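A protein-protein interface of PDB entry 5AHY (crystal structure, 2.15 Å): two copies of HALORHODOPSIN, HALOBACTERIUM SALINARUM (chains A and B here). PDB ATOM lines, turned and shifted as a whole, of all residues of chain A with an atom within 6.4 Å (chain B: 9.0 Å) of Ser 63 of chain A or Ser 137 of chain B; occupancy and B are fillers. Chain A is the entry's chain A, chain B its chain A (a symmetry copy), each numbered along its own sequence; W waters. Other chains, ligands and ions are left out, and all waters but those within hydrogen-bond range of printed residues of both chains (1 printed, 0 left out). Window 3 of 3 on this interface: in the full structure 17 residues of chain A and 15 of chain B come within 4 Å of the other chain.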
ATOM      1  N   TYR A  58     -18.451 -20.390   4.234  1.00  0.00           N
ATOM      2  CA  TYR A  58     -18.714 -20.446   2.803  1.00  0.00           C
ATOM      3  C   TYR A  58     -18.273 -19.164   2.102  1.00  0.00           C
ATOM      4  O   TYR A  58     -17.850 -19.213   0.961  1.00  0.00           O
ATOM      5  CB  TYR A  58     -20.205 -20.752   2.534  1.00  0.00           C
ATOM      6  CG  TYR A  58     -20.479 -22.243   2.675  1.00  0.00           C
ATOM      7  CD1 TYR A  58     -20.123 -23.134   1.652  1.00  0.00           C
ATOM      8  CD2 TYR A  58     -21.022 -22.773   3.850  1.00  0.00           C
ATOM      9  CE1 TYR A  58     -20.334 -24.513   1.777  1.00  0.00           C
ATOM     10  CE2 TYR A  58     -21.232 -24.162   3.988  1.00  0.00           C
ATOM     11  CZ  TYR A  58     -20.887 -25.016   2.943  1.00  0.00           C
ATOM     12  OH  TYR A  58     -21.102 -26.370   3.053  1.00  0.00           O
ATOM     13  N   LEU A  59     -18.361 -18.022   2.774  1.00  0.00           N
ATOM     14  CA  LEU A  59     -17.815 -16.798   2.186  1.00  0.00           C
ATOM     15  C   LEU A  59     -16.280 -16.870   2.140  1.00  0.00           C
ATOM     16  O   LEU A  59     -15.657 -16.372   1.210  1.00  0.00           O
ATOM     17  CB  LEU A  59     -18.262 -15.570   2.969  1.00  0.00           C
ATOM     18  CG  LEU A  59     -19.766 -15.274   2.921  1.00  0.00           C
ATOM     19  CD1 LEU A  59     -20.133 -14.408   4.106  1.00  0.00           C
ATOM     20  CD2 LEU A  59     -20.156 -14.590   1.600  1.00  0.00           C
ATOM     21  N   GLY A  60     -15.679 -17.493   3.153  1.00  0.00           N
ATOM     22  CA  GLY A  60     -14.248 -17.749   3.147  1.00  0.00           C
ATOM     23  C   GLY A  60     -13.837 -18.504   1.897  1.00  0.00           C
ATOM     24  O   GLY A  60     -12.871 -18.128   1.225  1.00  0.00           O
ATOM     25  N   LEU A  61     -14.591 -19.554   1.562  1.00  0.00           N
ATOM     26  CA  LEU A  61     -14.279 -20.365   0.386  1.00  0.00           C
ATOM     27  C   LEU A  61     -14.566 -19.623  -0.919  1.00  0.00           C
ATOM     28  O   LEU A  61     -13.755 -19.651  -1.843  1.00  0.00           O
ATOM     29  CB  LEU A  61     -15.057 -21.685   0.424  1.00  0.00           C
ATOM     30  CG  LEU A  61     -14.811 -22.597   1.631  1.00  0.00           C
ATOM     31  CD1 LEU A  61     -15.832 -23.736   1.689  1.00  0.00           C
ATOM     32  CD2 LEU A  61     -13.396 -23.166   1.607  1.00  0.00           C
ATOM     33  N   LEU A  62     -15.709 -18.950  -0.993  1.00  0.00           N
ATOM     34  CA  LEU A  62     -16.111 -18.250  -2.231  1.00  0.00           C
ATOM     35  C   LEU A  62     -15.151 -17.140  -2.641  1.00  0.00           C
ATOM     36  O   LEU A  62     -14.879 -16.939  -3.814  1.00  0.00           O
ATOM     37  CB  LEU A  62     -17.504 -17.645  -2.073  1.00  0.00           C
ATOM     38  CG  LEU A  62     -18.678 -18.528  -2.451  1.00  0.00           C
ATOM     39  CD1 LEU A  62     -19.954 -17.893  -1.952  1.00  0.00           C
ATOM     40  CD2 LEU A  62     -18.689 -18.674  -3.974  1.00  0.00           C
ATOM     41  N   SER A  63     -14.654 -16.421  -1.647  1.00  0.00           N
ATOM     42  CA  SER A  63     -13.744 -15.310  -1.849  1.00  0.00           C
ATOM     43  C   SER A  63     -12.300 -15.720  -2.191  1.00  0.00           C
ATOM     44  O   SER A  63     -11.463 -14.861  -2.449  1.00  0.00           O
ATOM     45  CB  SER A  63     -13.734 -14.432  -0.591  1.00  0.00           C
ATOM     46  OG  SER A  63     -13.171 -15.114   0.519  1.00  0.00           O
ATOM     47  N   GLY A  64     -12.009 -17.019  -2.177  1.00  0.00           N
ATOM     48  CA  GLY A  64     -10.650 -17.494  -2.381  1.00  0.00           C
ATOM     49  C   GLY A  64      -9.752 -17.434  -1.151  1.00  0.00           C
ATOM     50  O   GLY A  64      -8.651 -18.001  -1.138  1.00  0.00           O
ATOM     51  N   LEU A  65     -10.227 -16.760  -0.109  1.00  0.00           N
ATOM     52  CA  LEU A  65      -9.451 -16.572   1.110  1.00  0.00           C
ATOM     53  C   LEU A  65      -8.972 -17.872   1.738  1.00  0.00           C
ATOM     54  O   LEU A  65      -7.822 -17.962   2.180  1.00  0.00           O
ATOM     55  CB  LEU A  65     -10.273 -15.797   2.139  1.00  0.00           C
ATOM     56  CG  LEU A  65      -9.528 -15.308   3.383  1.00  0.00           C
ATOM     57  CD1 LEU A  65      -8.435 -14.297   3.012  1.00  0.00           C
ATOM     58  CD2 LEU A  65     -10.505 -14.688   4.348  1.00  0.00           C
ATOM     59  N   THR A  66      -9.849 -18.871   1.795  1.00  0.00           N
ATOM     60  CA  THR A  66      -9.529 -20.113   2.506  1.00  0.00           C
ATOM     61  C   THR A  66      -9.533 -21.336   1.592  1.00  0.00           C
ATOM     62  O   THR A  66      -9.874 -22.443   2.019  1.00  0.00           O
ATOM     63  CB  THR A  66     -10.506 -20.371   3.669  1.00  0.00           C
ATOM     64  OG1 THR A  66     -11.841 -20.521   3.158  1.00  0.00           O
ATOM     65  CG2 THR A  66     -10.468 -19.235   4.678  1.00  0.00           C
ATOM     66  N   ILE B  70      -1.869  -5.245   1.933  1.00  0.00           N
ATOM     67  CA  ILE B  70      -3.022  -5.860   1.303  1.00  0.00           C
ATOM     68  C   ILE B  70      -3.453  -5.066   0.058  1.00  0.00           C
ATOM     69  O   ILE B  70      -3.652  -3.845   0.111  1.00  0.00           O
ATOM     70  CB  ILE B  70      -4.225  -5.960   2.291  1.00  0.00           C
ATOM     71  CG1 ILE B  70      -3.818  -6.621   3.616  1.00  0.00           C
ATOM     72  CG2 ILE B  70      -5.376  -6.722   1.669  1.00  0.00           C
ATOM     73  CD1 ILE B  70      -3.465  -8.094   3.511  1.00  0.00           C
ATOM     74  N   GLU B  71      -3.597  -5.757  -1.062  1.00  0.00           N
ATOM     75  CA  GLU B  71      -4.037  -5.098  -2.297  1.00  0.00           C
ATOM     76  C   GLU B  71      -5.554  -4.887  -2.320  1.00  0.00           C
ATOM     77  O   GLU B  71      -6.321  -5.845  -2.247  1.00  0.00           O
ATOM     78  CB  GLU B  71      -3.619  -5.913  -3.519  1.00  0.00           C
ATOM     79  CG  GLU B  71      -3.915  -5.195  -4.829  1.00  0.00           C
ATOM     80  CD  GLU B  71      -3.556  -6.016  -6.052  1.00  0.00           C
ATOM     81  OE1 GLU B  71      -2.988  -7.122  -5.903  1.00  0.00           O
ATOM     82  OE2 GLU B  71      -3.857  -5.554  -7.169  1.00  0.00           O
ATOM     83  N   MET B  72      -5.990  -3.637  -2.416  1.00  0.00           N
ATOM     84  CA  MET B  72      -7.421  -3.352  -2.438  1.00  0.00           C
ATOM     85  C   MET B  72      -8.019  -3.736  -3.792  1.00  0.00           C
ATOM     86  O   MET B  72      -7.403  -3.509  -4.835  1.00  0.00           O
ATOM     87  CB  MET B  72      -7.685  -1.882  -2.116  1.00  0.00           C
ATOM     88  CG  MET B  72      -7.270  -1.465  -0.699  1.00  0.00           C
ATOM     89  SD  MET B  72      -8.152  -2.312   0.647  1.00  0.00           S
ATOM     90  CE  MET B  72      -7.052  -3.692   1.003  1.00  0.00           C
ATOM     91  N   PRO B  73      -9.216  -4.342  -3.773  1.00  0.00           N
ATOM     92  CA  PRO B  73      -9.863  -4.854  -4.990  1.00  0.00           C
ATOM     93  C   PRO B  73     -10.567  -3.744  -5.753  1.00  0.00           C
ATOM     94  O   PRO B  73     -10.829  -2.681  -5.181  1.00  0.00           O
ATOM     95  CB  PRO B  73     -10.883  -5.854  -4.439  1.00  0.00           C
ATOM     96  CG  PRO B  73     -11.327  -5.195  -3.170  1.00  0.00           C
ATOM     97  CD  PRO B  73     -10.058  -4.571  -2.583  1.00  0.00           C
ATOM     98  N   ALA B  74     -10.876  -4.001  -7.021  1.00  0.00           N
ATOM     99  CA  ALA B  74     -11.634  -3.063  -7.852  1.00  0.00           C
ATOM    100  C   ALA B  74     -12.871  -2.528  -7.148  1.00  0.00           C
ATOM    101  O   ALA B  74     -13.644  -3.285  -6.549  1.00  0.00           O
ATOM    102  CB  ALA B  74     -12.033  -3.733  -9.159  1.00  0.00           C
ATOM    103  N   GLY B  75     -13.060  -1.220  -7.224  1.00  0.00           N
ATOM    104  CA  GLY B  75     -14.210  -0.587  -6.605  1.00  0.00           C
ATOM    105  C   GLY B  75     -13.839   0.127  -5.325  1.00  0.00           C
ATOM    106  O   GLY B  75     -14.500   1.086  -4.923  1.00  0.00           O
ATOM    107  N   ALA B 131     -11.149 -11.582   8.479  1.00  0.00           N
ATOM    108  CA  ALA B 131     -11.421 -12.043   7.115  1.00  0.00           C
ATOM    109  C   ALA B 131     -11.707 -10.875   6.171  1.00  0.00           C
ATOM    110  O   ALA B 131     -11.239 -10.867   5.028  1.00  0.00           O
ATOM    111  CB  ALA B 131     -12.595 -13.026   7.113  1.00  0.00           C
ATOM    112  N   ALA B 132     -12.488  -9.910   6.659  1.00  0.00           N
ATOM    113  CA  ALA B 132     -12.847  -8.701   5.913  1.00  0.00           C
ATOM    114  C   ALA B 132     -11.632  -7.899   5.465  1.00  0.00           C
ATOM    115  O   ALA B 132     -11.584  -7.382   4.342  1.00  0.00           O
ATOM    116  CB  ALA B 132     -13.773  -7.811   6.771  1.00  0.00           C
ATOM    117  N   ALA B 133     -10.666  -7.769   6.368  1.00  0.00           N
ATOM    118  CA  ALA B 133      -9.439  -7.027   6.097  1.00  0.00           C
ATOM    119  C   ALA B 133      -8.529  -7.807   5.157  1.00  0.00           C
ATOM    120  O   ALA B 133      -7.847  -7.219   4.314  1.00  0.00           O
ATOM    121  CB  ALA B 133      -8.705  -6.707   7.425  1.00  0.00           C
ATOM    122  N   MET B 134      -8.538  -9.135   5.280  1.00  0.00           N
ATOM    123  CA  MET B 134      -7.633  -9.975   4.498  1.00  0.00           C
ATOM    124  C   MET B 134      -8.148 -10.281   3.090  1.00  0.00           C
ATOM    125  O   MET B 134      -7.383 -10.687   2.237  1.00  0.00           O
ATOM    126  CB  MET B 134      -7.348 -11.298   5.229  1.00  0.00           C
ATOM    127  CG  MET B 134      -6.583 -11.164   6.558  1.00  0.00           C
ATOM    128  SD  MET B 134      -4.973 -10.372   6.397  1.00  0.00           S
ATOM    129  CE  MET B 134      -5.359  -8.654   6.721  1.00  0.00           C
ATOM    130  N   THR B 135      -9.439 -10.090   2.846  1.00  0.00           N
ATOM    131  CA  THR B 135     -10.021 -10.462   1.561  1.00  0.00           C
ATOM    132  C   THR B 135      -9.643  -9.492   0.423  1.00  0.00           C
ATOM    133  O   THR B 135      -9.874  -8.285   0.517  1.00  0.00           O
ATOM    134  CB  THR B 135     -11.553 -10.558   1.667  1.00  0.00           C
ATOM    135  OG1 THR B 135     -11.902 -11.655   2.528  1.00  0.00           O
ATOM    136  CG2 THR B 135     -12.168 -10.797   0.285  1.00  0.00           C
ATOM    137  N   THR B 136      -9.064 -10.037  -0.648  1.00  0.00           N
ATOM    138  CA  THR B 136      -8.620  -9.244  -1.791  1.00  0.00           C
ATOM    139  C   THR B 136      -9.351  -9.504  -3.114  1.00  0.00           C
ATOM    140  O   THR B 136      -9.238  -8.697  -4.021  1.00  0.00           O
ATOM    141  CB  THR B 136      -7.136  -9.473  -2.095  1.00  0.00           C
ATOM    142  OG1 THR B 136      -6.921 -10.866  -2.342  1.00  0.00           O
ATOM    143  CG2 THR B 136      -6.268  -9.014  -0.934  1.00  0.00           C
ATOM    144  N   SER B 137     -10.057 -10.630  -3.245  1.00  0.00           N
ATOM    145  CA  SER B 137     -10.665 -10.998  -4.530  1.00  0.00           C
ATOM    146  C   SER B 137     -11.766 -10.024  -4.985  1.00  0.00           C
ATOM    147  O   SER B 137     -11.860  -9.691  -6.150  1.00  0.00           O
ATOM    148  CB  SER B 137     -11.236 -12.430  -4.459  1.00  0.00           C
ATOM    149  OG  SER B 137     -12.127 -12.591  -3.354  1.00  0.00           O
ATOM    150  N   ALA B 138     -12.605  -9.576  -4.062  1.00  0.00           N
ATOM    151  CA  ALA B 138     -13.727  -8.726  -4.430  1.00  0.00           C
ATOM    152  C   ALA B 138     -14.140  -7.832  -3.278  1.00  0.00           C
ATOM    153  O   ALA B 138     -14.106  -8.241  -2.111  1.00  0.00           O
ATOM    154  CB  ALA B 138     -14.924  -9.587  -4.894  1.00  0.00           C
ATOM    155  N   LEU B 139     -14.548  -6.612  -3.617  1.00  0.00           N
ATOM    156  CA  LEU B 139     -15.076  -5.653  -2.649  1.00  0.00           C
ATOM    157  C   LEU B 139     -16.337  -6.165  -1.917  1.00  0.00           C
ATOM    158  O   LEU B 139     -16.513  -5.904  -0.730  1.00  0.00           O
ATOM    159  CB  LEU B 139     -15.380  -4.335  -3.361  1.00  0.00           C
ATOM    160  CG  LEU B 139     -15.644  -3.098  -2.506  1.00  0.00           C
ATOM    161  CD1 LEU B 139     -14.449  -2.821  -1.624  1.00  0.00           C
ATOM    162  CD2 LEU B 139     -15.936  -1.892  -3.402  1.00  0.00           C
ATOM    163  N   LEU B 140     -17.194  -6.895  -2.636  1.00  0.00           N
ATOM    164  CA  LEU B 140     -18.412  -7.513  -2.080  1.00  0.00           C
ATOM    165  C   LEU B 140     -18.167  -8.406  -0.865  1.00  0.00           C
ATOM    166  O   LEU B 140     -18.883  -8.324   0.144  1.00  0.00           O
ATOM    167  CB  LEU B 140     -19.113  -8.360  -3.159  1.00  0.00           C
ATOM    168  CG  LEU B 140     -20.186  -9.347  -2.662  1.00  0.00           C
ATOM    169  CD1 LEU B 140     -21.442  -8.602  -2.265  1.00  0.00           C
ATOM    170  CD2 LEU B 140     -20.504 -10.410  -3.706  1.00  0.00           C
ATOM    171  N   PHE B 141     -17.171  -9.282  -0.998  1.00  0.00           N
ATOM    172  CA  PHE B 141     -16.803 -10.231   0.045  1.00  0.00           C
ATOM    173  C   PHE B 141     -16.226  -9.525   1.268  1.00  0.00           C
ATOM    174  O   PHE B 141     -16.472  -9.949   2.391  1.00  0.00           O
ATOM    175  CB  PHE B 141     -15.808 -11.263  -0.502  1.00  0.00           C
ATOM    176  CG  PHE B 141     -16.422 -12.225  -1.486  1.00  0.00           C
ATOM    177  CD1 PHE B 141     -17.554 -12.956  -1.144  1.00  0.00           C
ATOM    178  CD2 PHE B 141     -15.890 -12.378  -2.751  1.00  0.00           C
ATOM    179  CE1 PHE B 141     -18.137 -13.831  -2.047  1.00  0.00           C
ATOM    180  CE2 PHE B 141     -16.470 -13.254  -3.671  1.00  0.00           C
ATOM    181  CZ  PHE B 141     -17.593 -13.982  -3.313  1.00  0.00           C
ATOM    182  N   ARG B 142     -15.479  -8.439   1.063  1.00  0.00           N
ATOM    183  CA  ARG B 142     -14.983  -7.677   2.207  1.00  0.00           C
ATOM    184  C   ARG B 142     -16.152  -7.202   3.077  1.00  0.00           C
ATOM    185  O   ARG B 142     -16.155  -7.398   4.294  1.00  0.00           O
ATOM    186  CB  ARG B 142     -14.130  -6.484   1.749  1.00  0.00           C
ATOM    187  CG  ARG B 142     -12.748  -6.878   1.211  1.00  0.00           C
ATOM    188  CD  ARG B 142     -11.950  -5.661   0.729  1.00  0.00           C
ATOM    189  NE  ARG B 142     -11.523  -4.771   1.814  1.00  0.00           N
ATOM    190  CZ  ARG B 142     -10.402  -4.934   2.524  1.00  0.00           C
ATOM    191  NH1 ARG B 142      -9.611  -5.967   2.283  1.00  0.00           N
ATOM    192  NH2 ARG B 142     -10.084  -4.078   3.493  1.00  0.00           N
ATOM    193  N   ALA B 144     -19.324  -8.222   2.981  1.00  0.00           N
ATOM    194  CA  ALA B 144     -20.120  -9.349   3.457  1.00  0.00           C
ATOM    195  C   ALA B 144     -19.558  -9.870   4.786  1.00  0.00           C
ATOM    196  O   ALA B 144     -20.312 -10.152   5.713  1.00  0.00           O
ATOM    197  CB  ALA B 144     -20.157 -10.460   2.417  1.00  0.00           C
ATOM    198  N   PHE B 145     -18.236  -9.997   4.873  1.00  0.00           N
ATOM    199  CA  PHE B 145     -17.580 -10.377   6.133  1.00  0.00           C
ATOM    200  C   PHE B 145     -17.829  -9.339   7.229  1.00  0.00           C
ATOM    201  O   PHE B 145     -18.106  -9.699   8.380  1.00  0.00           O
ATOM    202  CB  PHE B 145     -16.067 -10.573   5.926  1.00  0.00           C
ATOM    203  CG  PHE B 145     -15.695 -11.943   5.436  1.00  0.00           C
ATOM    204  CD1 PHE B 145     -16.158 -13.077   6.097  1.00  0.00           C
ATOM    205  CD2 PHE B 145     -14.897 -12.102   4.313  1.00  0.00           C
ATOM    206  CE1 PHE B 145     -15.829 -14.352   5.652  1.00  0.00           C
ATOM    207  CE2 PHE B 145     -14.564 -13.377   3.848  1.00  0.00           C
ATOM    208  CZ  PHE B 145     -15.030 -14.503   4.525  1.00  0.00           C
HETATM  209  O   HOH W   1      -9.803 -12.990  -1.322  1.00  0.00           O
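The backbone carbonyl oxygen (O) of Ser 63 of chain A lies within hydrogen-bond range of the side-chain hydroxyl (OG) of Ser 137 of chain B, at 2.5 Å.
Among the printed residues, pairs that only touch across the chains: Leu 59 of chain A with Phe 145 of chain B, Gly 60 of chain A with Phe 145 of chain B, Leu 62 of chain A with Phe 141 of chain B, Ser 63 of chain A with Phe 141 of chain B, Leu 65 of chain A with Ala 131 of chain B, Leu 65 of chain A with Met 134 of chain B and Leu 65 of chain A with Thr 135 of chain B.
The backbone carbonyl oxygen (O) of Leu 59 of chain A is in hydrogen-bond range of the side-chain hydroxyl (OG) of Ser 63 of chain A (2.9 Å). OG of Ser 63 of chain A sits at hydrogen-bond distance from O of Gly 60 of chain A (3.1 Å). The backbone carbonyl oxygen (O) of Gly 60 of chain A lies within hydrogen-bond range of the backbone NH (N) of Leu 65 of chain A (3.3 Å). The backbone carbonyl oxygen of Gly 60 of chain A is in hydrogen-bond range of the backbone NH of Thr 66 of chain A (3.2 Å). The side-chain hydroxyl (OG) of Ser 63 of chain A lies close to the backbone NH (N) of Leu 65 of chain A, at 3.4 Å. The side-chain hydroxyl of Thr 135 of chain B lies within hydrogen-bond range of the backbone carbonyl oxygen of Ala 131 of chain B, at 2.7 Å.
Water W1 lies within hydrogen-bond range of O of Ser 63 of chain A (2.7 Å), N of Ser 137 of chain B (3.1 Å) and N of Thr 136 of chain B (3.1 Å).
Hydrophobic or aromatic side chains of chain A within 4 Å of the printed part of chain B: Leu 59, Leu 62 and Leu 65. Of the 20 printed residues of chain B, 6 touch a printed residue of chain A. Hydrophobic or aromatic side chains of chain B that line the printed part of chain A: Ala 131, Met 134, Phe 141 and Phe 145.
No position is printed for both chains. Of the 8 pairs that touch across the chains among the printed residues, none has its exchanged pair printed and touching as well.
Of chain B, only Phe 145 (3.4 Å) comes within 4 Å of Gly 60 of chain A. Of the printed residues of chain B, Leu 62 of chain A touches Phe 141 (3.9 Å). Printed residues of chain B within 4 Å of Ser 63 of chain A: Ser 137 (2.5 Å) and Phe 141 (3.6 Å). No residue of chain B comes within 4 Å of Gly 64 of chain A. Of the printed residues of chain A, Ala 131 of chain B touches Leu 65. Of the printed residues of chain A, Met 134 of chain B touches Leu 65 (3.8 Å). Ser 137 of chain B touches one residue of chain A. Printed residues of chain A within 4 Å of Phe 141 of chain B: Leu 62 (3.9 Å) and Ser 63 (3.6 Å). The nearest printed residue of chain B that does not touch Ser 63 of chain A is Phe 145 of chain B (4.005 Å).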
